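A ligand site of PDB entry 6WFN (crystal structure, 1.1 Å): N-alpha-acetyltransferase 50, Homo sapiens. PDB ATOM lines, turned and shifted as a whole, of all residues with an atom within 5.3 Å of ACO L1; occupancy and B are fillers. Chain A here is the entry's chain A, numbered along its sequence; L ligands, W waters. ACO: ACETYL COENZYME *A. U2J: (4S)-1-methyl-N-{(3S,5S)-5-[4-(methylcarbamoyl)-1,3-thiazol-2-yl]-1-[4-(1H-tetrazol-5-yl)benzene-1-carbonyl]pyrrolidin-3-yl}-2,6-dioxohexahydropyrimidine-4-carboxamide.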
ATOM      1  N   ILE A  28      17.471  15.190  13.158  1.00  0.00           N
ATOM      2  CA  ILE A  28      16.259  15.864  13.561  1.00  0.00           C
ATOM      3  C   ILE A  28      15.580  15.289  14.768  1.00  0.00           C
ATOM      4  O   ILE A  28      15.087  16.045  15.584  1.00  0.00           O
ATOM      5  CB  ILE A  28      15.266  15.927  12.368  1.00  0.00           C
ATOM      6  CG1 ILE A  28      15.885  16.791  11.229  1.00  0.00           C
ATOM      7  CG2 ILE A  28      13.885  16.464  12.763  1.00  0.00           C
ATOM      8  CD1 ILE A  28      15.192  16.528   9.835  1.00  0.00           C
ATOM      9  N   PHE A  29      15.499  13.974  14.868  1.00  0.00           N
ATOM     10  CA  PHE A  29      14.683  13.343  15.906  1.00  0.00           C
ATOM     11  C   PHE A  29      15.483  12.881  17.107  1.00  0.00           C
ATOM     12  O   PHE A  29      16.673  12.564  16.957  1.00  0.00           O
ATOM     13  CB  PHE A  29      13.878  12.169  15.298  1.00  0.00           C
ATOM     14  CG  PHE A  29      12.957  12.644  14.189  1.00  0.00           C
ATOM     15  CD1 PHE A  29      11.793  13.356  14.482  1.00  0.00           C
ATOM     16  CD2 PHE A  29      13.280  12.433  12.871  1.00  0.00           C
ATOM     17  CE1 PHE A  29      10.979  13.835  13.435  1.00  0.00           C
ATOM     18  CE2 PHE A  29      12.488  12.958  11.843  1.00  0.00           C
ATOM     19  CZ  PHE A  29      11.350  13.656  12.146  1.00  0.00           C
ATOM     20  N   ILE A  76       1.734   8.586   9.949  1.00  0.00           N
ATOM     21  CA  ILE A  76       2.927   9.392   9.715  1.00  0.00           C
ATOM     22  C   ILE A  76       3.945   9.007  10.774  1.00  0.00           C
ATOM     23  O   ILE A  76       3.704   9.292  11.961  1.00  0.00           O
ATOM     24  CB  ILE A  76       2.624  10.885   9.755  1.00  0.00           C
ATOM     25  CG1 ILE A  76       1.518  11.300   8.769  1.00  0.00           C
ATOM     26  CG2 ILE A  76       3.928  11.648   9.468  1.00  0.00           C
ATOM     27  CD1 ILE A  76       1.147  12.771   8.837  1.00  0.00           C
ATOM     28  N   MET A  77       5.038   8.378  10.388  1.00  0.00           N
ATOM     29  CA  MET A  77       6.046   7.957  11.347  1.00  0.00           C
ATOM     30  C   MET A  77       7.016   9.066  11.698  1.00  0.00           C
ATOM     31  O   MET A  77       7.311   9.300  12.877  1.00  0.00           O
ATOM     32  CB  MET A  77       6.815   6.751  10.795  1.00  0.00           C
ATOM     33  CG  MET A  77       5.942   5.531  10.655  1.00  0.00           C
ATOM     34  SD  MET A  77       6.723   4.086   9.951  1.00  0.00           S
ATOM     35  CE  MET A  77       6.864   4.640   8.250  1.00  0.00           C
ATOM     36  N   THR A  78       7.503   9.772  10.672  1.00  0.00           N
ATOM     37  CA  THR A  78       8.453  10.849  10.866  1.00  0.00           C
ATOM     38  C   THR A  78       8.130  11.976   9.888  1.00  0.00           C
ATOM     39  O   THR A  78       7.812  11.695   8.722  1.00  0.00           O
ATOM     40  CB  THR A  78       9.925  10.403  10.718  1.00  0.00           C
ATOM     41  OG1 THR A  78      10.150   9.810   9.455  1.00  0.00           O
ATOM     42  CG2 THR A  78      10.364   9.430  11.791  1.00  0.00           C
ATOM     43  N   LEU A  79       8.248  13.228  10.317  1.00  0.00           N
ATOM     44  CA  LEU A  79       8.082  14.370   9.442  1.00  0.00           C
ATOM     45  C   LEU A  79       8.897  15.460  10.076  1.00  0.00           C
ATOM     46  O   LEU A  79       8.658  15.817  11.231  1.00  0.00           O
ATOM     47  CB  LEU A  79       6.603  14.746   9.299  1.00  0.00           C
ATOM     48  CG  LEU A  79       6.268  15.815   8.274  1.00  0.00           C
ATOM     49  CD1 LEU A  79       4.800  15.733   7.898  1.00  0.00           C
ATOM     50  CD2 LEU A  79       6.557  17.212   8.820  1.00  0.00           C
ATOM     51  N   GLY A  80       9.916  15.952   9.385  1.00  0.00           N
ATOM     52  CA  GLY A  80      10.752  16.959  10.018  1.00  0.00           C
ATOM     53  C   GLY A  80      11.643  17.639   9.029  1.00  0.00           C
ATOM     54  O   GLY A  80      11.892  17.179   7.923  1.00  0.00           O
ATOM     55  N   CYS A  81      12.203  18.759   9.523  1.00  0.00           N
ATOM     56  CA  CYS A  81      13.035  19.652   8.743  1.00  0.00           C
ATOM     57  C   CYS A  81      14.287  19.989   9.611  1.00  0.00           C
ATOM     58  O   CYS A  81      14.130  20.212  10.810  1.00  0.00           O
ATOM     59  CB  CYS A  81      12.164  20.889   8.474  1.00  0.00           C
ATOM     60  SG  CYS A  81      12.923  22.155   7.436  1.00  0.00           S
ATOM     61  N   TYR A  85      16.350  25.387   8.343  1.00  0.00           N
ATOM     62  CA  TYR A  85      15.412  25.551   7.244  1.00  0.00           C
ATOM     63  C   TYR A  85      13.963  25.570   7.675  1.00  0.00           C
ATOM     64  O   TYR A  85      13.077  25.557   6.824  1.00  0.00           O
ATOM     65  CB  TYR A  85      15.667  24.451   6.215  1.00  0.00           C
ATOM     66  CG  TYR A  85      17.106  24.423   5.779  1.00  0.00           C
ATOM     67  CD1 TYR A  85      18.044  23.638   6.440  1.00  0.00           C
ATOM     68  CD2 TYR A  85      17.546  25.167   4.693  1.00  0.00           C
ATOM     69  CE1 TYR A  85      19.375  23.602   6.060  1.00  0.00           C
ATOM     70  CE2 TYR A  85      18.885  25.141   4.294  1.00  0.00           C
ATOM     71  CZ  TYR A  85      19.791  24.360   4.985  1.00  0.00           C
ATOM     72  OH  TYR A  85      21.116  24.285   4.603  1.00  0.00           O
ATOM     73  N   ARG A  86      13.697  25.642   8.986  1.00  0.00           N
ATOM     74  CA  ARG A  86      12.329  25.669   9.491  1.00  0.00           C
ATOM     75  C   ARG A  86      11.654  26.990   9.221  1.00  0.00           C
ATOM     76  O   ARG A  86      12.308  28.002   8.949  1.00  0.00           O
ATOM     77  CB  ARG A  86      12.308  25.318  10.988  1.00  0.00           C
ATOM     78  CG  ARG A  86      12.638  23.873  11.204  1.00  0.00           C
ATOM     79  CD  ARG A  86      12.666  23.497  12.676  1.00  0.00           C
ATOM     80  NE  ARG A  86      13.275  22.180  12.750  1.00  0.00           N
ATOM     81  CZ  ARG A  86      13.808  21.638  13.830  1.00  0.00           C
ATOM     82  NH1 ARG A  86      13.720  22.266  15.006  1.00  0.00           N
ATOM     83  NH2 ARG A  86      14.466  20.491  13.759  1.00  0.00           N
ATOM     84  N   ARG A  87      10.338  27.005   9.275  1.00  0.00           N
ATOM     85  CA  ARG A  87       9.535  28.220   9.076  1.00  0.00           C
ATOM     86  C   ARG A  87       9.698  28.810   7.694  1.00  0.00           C
ATOM     87  O   ARG A  87       9.650  30.034   7.503  1.00  0.00           O
ATOM     88  CB  ARG A  87       9.769  29.292  10.174  1.00  0.00           C
ATOM     89  CG  ARG A  87       9.243  28.953  11.553  1.00  0.00           C
ATOM     90  CD  ARG A  87       7.748  28.627  11.631  1.00  0.00           C
ATOM     91  NE  ARG A  87       6.805  29.746  11.562  1.00  0.00           N
ATOM     92  CZ  ARG A  87       6.506  30.560  12.568  1.00  0.00           C
ATOM     93  NH1 ARG A  87       7.181  30.491  13.715  1.00  0.00           N
ATOM     94  NH2 ARG A  87       5.555  31.460  12.435  1.00  0.00           N
ATOM     95  N   LEU A  88       9.862  27.923   6.701  1.00  0.00           N
ATOM     96  CA  LEU A  88       9.981  28.297   5.295  1.00  0.00           C
ATOM     97  C   LEU A  88       8.939  27.567   4.461  1.00  0.00           C
ATOM     98  O   LEU A  88       8.966  27.645   3.239  1.00  0.00           O
ATOM     99  CB  LEU A  88      11.396  28.013   4.769  1.00  0.00           C
ATOM    100  CG  LEU A  88      12.519  28.851   5.375  1.00  0.00           C
ATOM    101  CD1 LEU A  88      13.866  28.383   4.870  1.00  0.00           C
ATOM    102  CD2 LEU A  88      12.338  30.351   5.044  1.00  0.00           C
ATOM    103  N   GLY A  89       8.021  26.842   5.108  1.00  0.00           N
ATOM    104  CA  GLY A  89       6.949  26.121   4.413  1.00  0.00           C
ATOM    105  C   GLY A  89       7.294  24.694   4.034  1.00  0.00           C
ATOM    106  O   GLY A  89       6.483  24.039   3.362  1.00  0.00           O
ATOM    107  N   ILE A  90       8.438  24.172   4.459  1.00  0.00           N
ATOM    108  CA  ILE A  90       8.849  22.818   4.050  1.00  0.00           C
ATOM    109  C   ILE A  90       7.977  21.753   4.700  1.00  0.00           C
ATOM    110  O   ILE A  90       7.495  20.821   4.019  1.00  0.00           O
ATOM    111  CB  ILE A  90      10.345  22.607   4.325  1.00  0.00           C
ATOM    112  CG1 ILE A  90      11.186  23.593   3.472  1.00  0.00           C
ATOM    113  CG2 ILE A  90      10.733  21.139   4.103  1.00  0.00           C
ATOM    114  CD1 ILE A  90      12.648  23.660   3.718  1.00  0.00           C
ATOM    115  N   GLY A  91       7.680  21.911   5.986  1.00  0.00           N
ATOM    116  CA  GLY A  91       6.787  20.988   6.689  1.00  0.00           C
ATOM    117  C   GLY A  91       5.432  20.961   6.013  1.00  0.00           C
ATOM    118  O   GLY A  91       4.863  19.885   5.783  1.00  0.00           O
ATOM    119  N   THR A  92       4.906  22.154   5.673  1.00  0.00           N
ATOM    120  CA  THR A  92       3.631  22.269   4.982  1.00  0.00           C
ATOM    121  C   THR A  92       3.649  21.544   3.642  1.00  0.00           C
ATOM    122  O   THR A  92       2.722  20.812   3.323  1.00  0.00           O
ATOM    123  CB  THR A  92       3.196  23.725   4.843  1.00  0.00           C
ATOM    124  OG1 THR A  92       3.003  24.294   6.130  1.00  0.00           O
ATOM    125  CG2 THR A  92       1.928  23.914   4.024  1.00  0.00           C
ATOM    126  N   LYS A  93       4.701  21.731   2.862  1.00  0.00           N
ATOM    127  CA  LYS A  93       4.801  21.044   1.575  1.00  0.00           C
ATOM    128  C   LYS A  93       4.775  19.527   1.763  1.00  0.00           C
ATOM    129  O   LYS A  93       4.135  18.812   0.986  1.00  0.00           O
ATOM    130  CB  LYS A  93       6.073  21.483   0.853  1.00  0.00           C
ATOM    131  CG  LYS A  93       6.055  21.090  -0.602  1.00  0.00           C
ATOM    132  CD  LYS A  93       7.330  21.467  -1.300  1.00  0.00           C
ATOM    133  CE  LYS A  93       7.112  21.587  -2.798  1.00  0.00           C
ATOM    134  NZ  LYS A  93       6.713  20.298  -3.410  1.00  0.00           N
ATOM    135  N   LEU A 113      -0.654  10.044  13.968  1.00  0.00           N
ATOM    136  CA  LEU A 113       0.758  10.075  14.303  1.00  0.00           C
ATOM    137  C   LEU A 113       0.881  10.129  15.805  1.00  0.00           C
ATOM    138  O   LEU A 113      -0.082  10.497  16.512  1.00  0.00           O
ATOM    139  CB  LEU A 113       1.417  11.290  13.644  1.00  0.00           C
ATOM    140  CG  LEU A 113       0.899  12.658  14.086  1.00  0.00           C
ATOM    141  CD1 LEU A 113       1.648  13.253  15.292  1.00  0.00           C
ATOM    142  CD2 LEU A 113       0.826  13.605  12.950  1.00  0.00           C
ATOM    143  N   HIS A 114       2.083   9.890  16.299  1.00  0.00           N
ATOM    144  CA  HIS A 114       2.431  10.078  17.692  1.00  0.00           C
ATOM    145  C   HIS A 114       3.361  11.271  17.811  1.00  0.00           C
ATOM    146  O   HIS A 114       4.240  11.464  16.976  1.00  0.00           O
ATOM    147  CB  HIS A 114       3.169   8.840  18.220  1.00  0.00           C
ATOM    148  CG  HIS A 114       2.280   7.671  18.426  1.00  0.00           C
ATOM    149  ND1 HIS A 114       2.103   6.708  17.444  1.00  0.00           N
ATOM    150  CD2 HIS A 114       1.571   7.306  19.511  1.00  0.00           C
ATOM    151  CE1 HIS A 114       1.272   5.824  17.946  1.00  0.00           C
ATOM    152  NE2 HIS A 114       0.893   6.167  19.176  1.00  0.00           N
ATOM    153  N   VAL A 115       3.190  12.036  18.889  1.00  0.00           N
ATOM    154  CA  VAL A 115       4.080  13.138  19.165  1.00  0.00           C
ATOM    155  C   VAL A 115       4.316  13.268  20.656  1.00  0.00           C
ATOM    156  O   VAL A 115       3.381  13.266  21.455  1.00  0.00           O
ATOM    157  CB  VAL A 115       3.605  14.455  18.544  1.00  0.00           C
ATOM    158  CG1 VAL A 115       2.253  14.872  19.070  1.00  0.00           C
ATOM    159  CG2 VAL A 115       4.618  15.574  18.728  1.00  0.00           C
ATOM    160  N   ASN A 119       6.336  18.539  22.746  1.00  0.00           N
ATOM    161  CA  ASN A 119       6.585  19.204  21.480  1.00  0.00           C
ATOM    162  C   ASN A 119       5.406  20.063  21.079  1.00  0.00           C
ATOM    163  O   ASN A 119       4.647  19.762  20.153  1.00  0.00           O
ATOM    164  CB  ASN A 119       6.922  18.143  20.450  1.00  0.00           C
ATOM    165  CG  ASN A 119       7.569  18.703  19.231  1.00  0.00           C
ATOM    166  OD1 ASN A 119       7.492  19.894  18.934  1.00  0.00           O
ATOM    167  ND2 ASN A 119       8.244  17.840  18.465  1.00  0.00           N
ATOM    168  N   SER A 121       5.304  22.972  19.651  1.00  0.00           N
ATOM    169  CA  SER A 121       5.297  23.543  18.311  1.00  0.00           C
ATOM    170  C   SER A 121       4.832  22.551  17.252  1.00  0.00           C
ATOM    171  O   SER A 121       4.095  22.954  16.343  1.00  0.00           O
ATOM    172  CB  SER A 121       6.646  24.121  17.948  1.00  0.00           C
ATOM    173  OG  SER A 121       7.634  23.110  17.915  1.00  0.00           O
ATOM    174  N   ALA A 122       5.202  21.265  17.373  1.00  0.00           N
ATOM    175  CA  ALA A 122       4.711  20.295  16.389  1.00  0.00           C
ATOM    176  C   ALA A 122       3.205  20.099  16.546  1.00  0.00           C
ATOM    177  O   ALA A 122       2.493  20.026  15.559  1.00  0.00           O
ATOM    178  CB  ALA A 122       5.426  18.972  16.525  1.00  0.00           C
ATOM    179  N   PHE A 125       1.521  22.945  14.933  1.00  0.00           N
ATOM    180  CA  PHE A 125       1.670  22.822  13.483  1.00  0.00           C
ATOM    181  C   PHE A 125       0.594  21.876  12.907  1.00  0.00           C
ATOM    182  O   PHE A 125      -0.130  22.227  11.972  1.00  0.00           O
ATOM    183  CB  PHE A 125       3.103  22.357  13.149  1.00  0.00           C
ATOM    184  CG  PHE A 125       3.303  21.822  11.747  1.00  0.00           C
ATOM    185  CD1 PHE A 125       3.498  22.690  10.671  1.00  0.00           C
ATOM    186  CD2 PHE A 125       3.314  20.446  11.497  1.00  0.00           C
ATOM    187  CE1 PHE A 125       3.701  22.191   9.388  1.00  0.00           C
ATOM    188  CE2 PHE A 125       3.476  19.953  10.209  1.00  0.00           C
ATOM    189  CZ  PHE A 125       3.694  20.827   9.163  1.00  0.00           C
ATOM    190  N   TYR A 126       0.464  20.702  13.499  1.00  0.00           N
ATOM    191  CA  TYR A 126      -0.526  19.762  13.010  1.00  0.00           C
ATOM    192  C   TYR A 126      -1.954  20.220  13.217  1.00  0.00           C
ATOM    193  O   TYR A 126      -2.820  19.920  12.400  1.00  0.00           O
ATOM    194  CB  TYR A 126      -0.315  18.389  13.650  1.00  0.00           C
ATOM    195  CG  TYR A 126       0.895  17.658  13.118  1.00  0.00           C
ATOM    196  CD1 TYR A 126       0.924  17.143  11.832  1.00  0.00           C
ATOM    197  CD2 TYR A 126       1.997  17.442  13.939  1.00  0.00           C
ATOM    198  CE1 TYR A 126       2.046  16.462  11.352  1.00  0.00           C
ATOM    199  CE2 TYR A 126       3.102  16.753  13.473  1.00  0.00           C
ATOM    200  CZ  TYR A 126       3.147  16.306  12.170  1.00  0.00           C
ATOM    201  OH  TYR A 126       4.257  15.626  11.750  1.00  0.00           O
ATOM    202  N   LYS A 128      -3.172  23.025  12.767  1.00  0.00           N
ATOM    203  CA  LYS A 128      -3.516  23.907  11.636  1.00  0.00           C
ATOM    204  C   LYS A 128      -4.106  23.137  10.482  1.00  0.00           C
ATOM    205  O   LYS A 128      -4.828  23.726   9.661  1.00  0.00           O
ATOM    206  CB  LYS A 128      -2.250  24.622  11.121  1.00  0.00           C
ATOM    207  CG  LYS A 128      -1.663  25.568  12.152  1.00  0.00           C
ATOM    208  CD  LYS A 128      -0.495  26.327  11.600  1.00  0.00           C
ATOM    209  CE  LYS A 128      -0.958  27.565  10.887  1.00  0.00           C
ATOM    210  NZ  LYS A 128      -0.589  27.554   9.444  1.00  0.00           N
HETATM  211  N1A ACO L   1       6.211  28.316  16.220  1.00  0.00           N
HETATM  212  C2A ACO L   1       5.080  28.888  15.779  1.00  0.00           C
HETATM  213  N3A ACO L   1       4.363  28.587  14.686  1.00  0.00           N
HETATM  214  C4A ACO L   1       4.936  27.584  13.991  1.00  0.00           C
HETATM  215  C5A ACO L   1       6.110  26.920  14.312  1.00  0.00           C
HETATM  216  C6A ACO L   1       6.758  27.308  15.504  1.00  0.00           C
HETATM  217  N6A ACO L   1       7.842  26.691  15.993  1.00  0.00           N
HETATM  218  N7A ACO L   1       6.393  25.945  13.367  1.00  0.00           N
HETATM  219  C8A ACO L   1       5.384  26.018  12.531  1.00  0.00           C
HETATM  220  N9A ACO L   1       4.464  26.980  12.848  1.00  0.00           N
HETATM  221  C1B ACO L   1       3.176  27.216  12.181  1.00  0.00           C
HETATM  222  C2B ACO L   1       3.051  28.587  11.542  1.00  0.00           C
HETATM  223  O2B ACO L   1       1.691  28.992  11.551  1.00  0.00           O
HETATM  224  C3B ACO L   1       3.545  28.285  10.141  1.00  0.00           C
HETATM  225  O3B ACO L   1       3.071  29.211   9.141  1.00  0.00           O
HETATM  226  P3B ACO L   1       3.657  30.690   9.028  1.00  0.00           P
HETATM  227  O7A ACO L   1       3.209  31.178   7.735  1.00  0.00           O
HETATM  228  O8A ACO L   1       3.217  31.496  10.258  1.00  0.00           O
HETATM  229  O9A ACO L   1       5.103  30.564   9.100  1.00  0.00           O
HETATM  230  C4B ACO L   1       2.930  26.924   9.866  1.00  0.00           C
HETATM  231  O4B ACO L   1       2.990  26.257  11.142  1.00  0.00           O
HETATM  232  C5B ACO L   1       3.654  26.104   8.819  1.00  0.00           C
HETATM  233  O5B ACO L   1       5.033  25.997   9.186  1.00  0.00           O
HETATM  234  P1A ACO L   1       6.110  25.411   8.183  1.00  0.00           P
HETATM  235  O1A ACO L   1       7.075  26.454   7.816  1.00  0.00           O
HETATM  236  O2A ACO L   1       5.453  24.669   7.047  1.00  0.00           O
HETATM  237  O3A ACO L   1       6.756  24.332   9.155  1.00  0.00           O
HETATM  238  P2A ACO L   1       8.248  23.795   9.231  1.00  0.00           P
HETATM  239  O4A ACO L   1       8.813  23.603   7.855  1.00  0.00           O
HETATM  240  O5A ACO L   1       9.038  24.676  10.159  1.00  0.00           O
HETATM  241  O6A ACO L   1       8.018  22.391   9.853  1.00  0.00           O
HETATM  242  CBP ACO L   1       8.003  21.053  11.883  1.00  0.00           C
HETATM  243  CCP ACO L   1       7.343  22.187  11.109  1.00  0.00           C
HETATM  244  CDP ACO L   1       8.037  19.806  10.976  1.00  0.00           C
HETATM  245  CEP ACO L   1       7.158  20.771  13.129  1.00  0.00           C
HETATM  246  CAP ACO L   1       9.430  21.482  12.302  1.00  0.00           C
HETATM  247  OAP ACO L   1       9.338  22.448  13.363  1.00  0.00           O
HETATM  248  C9P ACO L   1      10.360  20.353  12.741  1.00  0.00           C
HETATM  249  O9P ACO L   1      10.948  19.675  11.907  1.00  0.00           O
HETATM  250  N8P ACO L   1      10.432  20.137  14.046  1.00  0.00           N
HETATM  251  C7P ACO L   1      11.294  19.113  14.618  1.00  0.00           C
HETATM  252  C6P ACO L   1      10.809  17.714  14.329  1.00  0.00           C
HETATM  253  C5P ACO L   1       9.356  17.565  14.677  1.00  0.00           C
HETATM  254  O5P ACO L   1       8.874  18.070  15.704  1.00  0.00           O
HETATM  255  N4P ACO L   1       8.611  16.877  13.816  1.00  0.00           N
HETATM  256  C3P ACO L   1       7.241  16.488  14.082  1.00  0.00           C
HETATM  257  C2P ACO L   1       7.238  15.382  15.128  1.00  0.00           C
HETATM  258  S1P ACO L   1       5.734  14.379  14.968  1.00  0.00           S
HETATM  259  C   ACO L   1       6.263  13.291  13.680  1.00  0.00           C
HETATM  260  O   ACO L   1       7.392  13.253  13.287  1.00  0.00           O
HETATM  261  CH3 ACO L   1       5.194  12.340  13.225  1.00  0.00           C
HETATM  262  C19 U2J L   2      11.303   4.824  18.867  1.00  0.00           C
HETATM  263  C21 U2J L   2       9.736   4.432  20.599  1.00  0.00           C
HETATM  264  C18 U2J L   2      10.331   4.573  17.923  1.00  0.00           C
HETATM  265  C22 U2J L   2       8.760   4.151  19.654  1.00  0.00           C
HETATM  266  C7  U2J L   2       8.461   2.201  12.810  1.00  0.00           C
HETATM  267  C20 U2J L   2      11.003   4.749  20.210  1.00  0.00           C
HETATM  268  C17 U2J L   2       9.067   4.235  18.324  1.00  0.00           C
HETATM  269  C6  U2J L   2       7.102   1.966  12.937  1.00  0.00           C
HETATM  270  C23 U2J L   2      12.059   5.026  21.228  1.00  0.00           C
HETATM  271  C5  U2J L   2       7.260   3.695  14.316  1.00  0.00           C
HETATM  272  C13 U2J L   2       9.737  11.125  16.724  1.00  0.00           C
HETATM  273  C14 U2J L   2       7.887  12.204  17.873  1.00  0.00           C
HETATM  274  C16 U2J L   2       8.025   3.966  17.300  1.00  0.00           C
HETATM  275  C8  U2J L   2       6.406   0.923  12.209  1.00  0.00           C
HETATM  276  C10 U2J L   2       7.157   9.371  16.488  1.00  0.00           C
HETATM  277  C12 U2J L   2       8.830  10.974  15.535  1.00  0.00           C
HETATM  278  C4  U2J L   2       6.707   6.130  14.694  1.00  0.00           C
HETATM  279  C2  U2J L   2       7.982   6.365  16.674  1.00  0.00           C
HETATM  280  C1  U2J L   2       6.857   4.737  15.289  1.00  0.00           C
HETATM  281  C11 U2J L   2       7.383  10.762  15.929  1.00  0.00           C
HETATM  282  C3  U2J L   2       6.848   7.019  15.909  1.00  0.00           C
HETATM  283  C15 U2J L   2      10.041  11.967  18.987  1.00  0.00           C
HETATM  284  C9  U2J L   2       4.422  -0.491  12.098  1.00  0.00           C
HETATM  285  N10 U2J L   2      11.803   5.371  22.505  1.00  0.00           N
HETATM  286  N2  U2J L   2       6.438   2.804  13.804  1.00  0.00           N
HETATM  287  N7  U2J L   2      13.350   4.984  20.919  1.00  0.00           N
HETATM  288  N9  U2J L   2      13.044   5.569  23.039  1.00  0.00           N
HETATM  289  N8  U2J L   2      13.958   5.327  22.086  1.00  0.00           N
HETATM  290  N6  U2J L   2       7.019  11.747  16.918  1.00  0.00           N
HETATM  291  N5  U2J L   2       9.177  11.709  17.816  1.00  0.00           N
HETATM  292  N1  U2J L   2       7.812   4.955  16.377  1.00  0.00           N
HETATM  293  N3  U2J L   2       5.115   0.702  12.555  1.00  0.00           N
HETATM  294  N4  U2J L   2       7.109   8.400  15.535  1.00  0.00           N
HETATM  295  O4  U2J L   2      10.914  10.755  16.698  1.00  0.00           O
HETATM  296  O3  U2J L   2       7.507  12.983  18.741  1.00  0.00           O
HETATM  297  O5  U2J L   2       7.462   2.883  17.223  1.00  0.00           O
HETATM  298  O1  U2J L   2       7.005   0.276  11.357  1.00  0.00           O
HETATM  299  O2  U2J L   2       7.039   9.104  17.679  1.00  0.00           O
HETATM  300  S1  U2J L   2       8.895   3.512  13.819  1.00  0.00           S
HETATM  301  O   HOH W   1       3.480  26.973  18.167  1.00  0.00           O
HETATM  302  O   HOH W   2       9.627  29.145  14.822  1.00  0.00           O
HETATM  303  O   HOH W   3       6.134  28.408  19.186  1.00  0.00           O
HETATM  304  O   HOH W   4       9.081  23.876  15.766  1.00  0.00           O
HETATM  305  O   HOH W   5       6.175  28.902   7.076  1.00  0.00           O
HETATM  306  O   HOH W   6       8.967  25.084  12.726  1.00  0.00           O
HETATM  307  O   HOH W   7       1.151  26.470  14.858  1.00  0.00           O
HETATM  308  O   HOH W   8       3.619  25.630  15.825  1.00  0.00           O
HETATM  309  O   HOH W   9       9.053  20.860  16.676  1.00  0.00           O
HETATM  310  O   HOH W  10      10.792  26.719  14.121  1.00  0.00           O
HETATM  311  O   HOH W  11       0.955  26.042   6.784  1.00  0.00           O
HETATM  312  O   HOH W  12       2.027  30.292  14.471  1.00  0.00           O
HETATM  313  O   HOH W  13       1.583  28.672   6.528  1.00  0.00           O
HETATM  314  O   HOH W  14      12.708  16.590  17.032  1.00  0.00           O
HETATM  315  O   HOH W  15       4.791  32.475   6.057  1.00  0.00           O
HETATM  316  O   HOH W  16      10.397  25.173   6.472  1.00  0.00           O
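An oxygen (O2A) of ACO L1 sits at hydrogen-bond distance from the backbone NH (N) of Thr 92.
OG1 of Thr 92 lies within hydrogen-bond range of O2A of ACO L1 (2.6 Å).
The backbone NH (N) of Gly 91 is in hydrogen-bond range of an oxygen (O4A) of ACO L1 (2.8 Å).
N of Leu 79 is in hydrogen-bond range of O of ACO L1 (3.1 Å).
O of Leu 79 is in hydrogen-bond range of N4P of ACO L1.
N of Arg 87 lies within hydrogen-bond range of O5A of ACO L1 (2.8 Å).
O9A of ACO L1 is in salt-bridge range of NE of Arg 87, at 3.1 Å.
An oxygen (O5P) of ACO L1 lies within hydrogen-bond range of the side-chain amide nitrogen (ND2) of Asn 119 (2.8 Å).
The backbone NH (N) of Cys 81 sits at hydrogen-bond distance from an oxygen (O9P) of ACO L1.
The backbone NH (N) of Gly 89 lies within hydrogen-bond range of an oxygen (O1A) of ACO L1, 2.9 Å away.
NZ of Lys 128 lies close to O2B of ACO L1.
N of Leu 88 is in hydrogen-bond range of O1A of ACO L1, 3.3 Å away.
The backbone NH (N) of Ile 90 lies within hydrogen-bond range of an oxygen (O4A) of ACO L1 (3.5 Å).
S1P of ACO L1 sits close to OH of Tyr 126, at 3.8 Å.
The backbone carbonyl oxygen (O) of Met 77 sits at hydrogen-bond distance from a nitrogen (N4) of U2J L2, at 2.8 Å.
The backbone carbonyl oxygen of His 114 lies within hydrogen-bond range of a nitrogen (N6) of U2J L2 (2.8 Å).
S1P of ACO L1 sits close to N6 of U2J L2, 3.5 Å away.
OD1 of Asn 119 lies within hydrogen-bond range of OG of Ser 121.
The backbone NH of Ala 122 lies within hydrogen-bond range of the side-chain amide oxygen of Asn 119 (3.1 Å).
The guanidinium group of Arg 86 sits at hydrogen-bond distance from the backbone carbonyl oxygen of Cys 81 (2.9 Å).
The backbone carbonyl oxygen (O) of Tyr 85 is in hydrogen-bond range of the side-chain sulfur (SG) of Cys 81 (3.5 Å).
Merely in contact with ACO L1: Gly 80 (3.3 Å), Arg 86 (3.4 Å), Ser 121 (3.4 Å), Thr 78 (3.6 Å), Ile 76 (3.6 Å), Phe 125 (3.6 Å), Phe 29 (3.6 Å), Ala 122 (3.7 Å), Ile 28 (3.7 Å), Met 77 (3.7 Å), His 114 (3.8 Å) and Leu 113 (3.9 Å).
Hydrophobic or aromatic side chains that line ACO L1: Ile 28, Phe 29, Leu 79, Ile 90, Leu 113, Ala 122, Phe 125 and Tyr 126.
The nearest printed residue that does not touch ACO L1 is Val 115 (4.1 Å).
Water W5 lies within hydrogen-bond range of O1A of ACO L1 (2.7 Å) and N of Gly 89 (3.4 Å).
Water W4 lies within hydrogen-bond range of OG of Ser 121 (2.7 Å) and OAP of ACO L1 (2.8 Å).
Water W9 lies within hydrogen-bond range of OD1 of Asn 119, OG of Ser 121 and O5P of ACO L1.
Water W8 lies within hydrogen-bond range of the backbone carbonyl oxygen of Ser 121 (2.8 Å) and a nitrogen (N3A) of ACO L1 (3.3 Å).
Water W2 bridges the guanidinium group of Arg 87 and a nitrogen (N6A) of ACO L1.
Water W11 lies within hydrogen-bond range of OG1 of Thr 92 (2.8 Å) and NZ of Lys 128 (3.4 Å).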
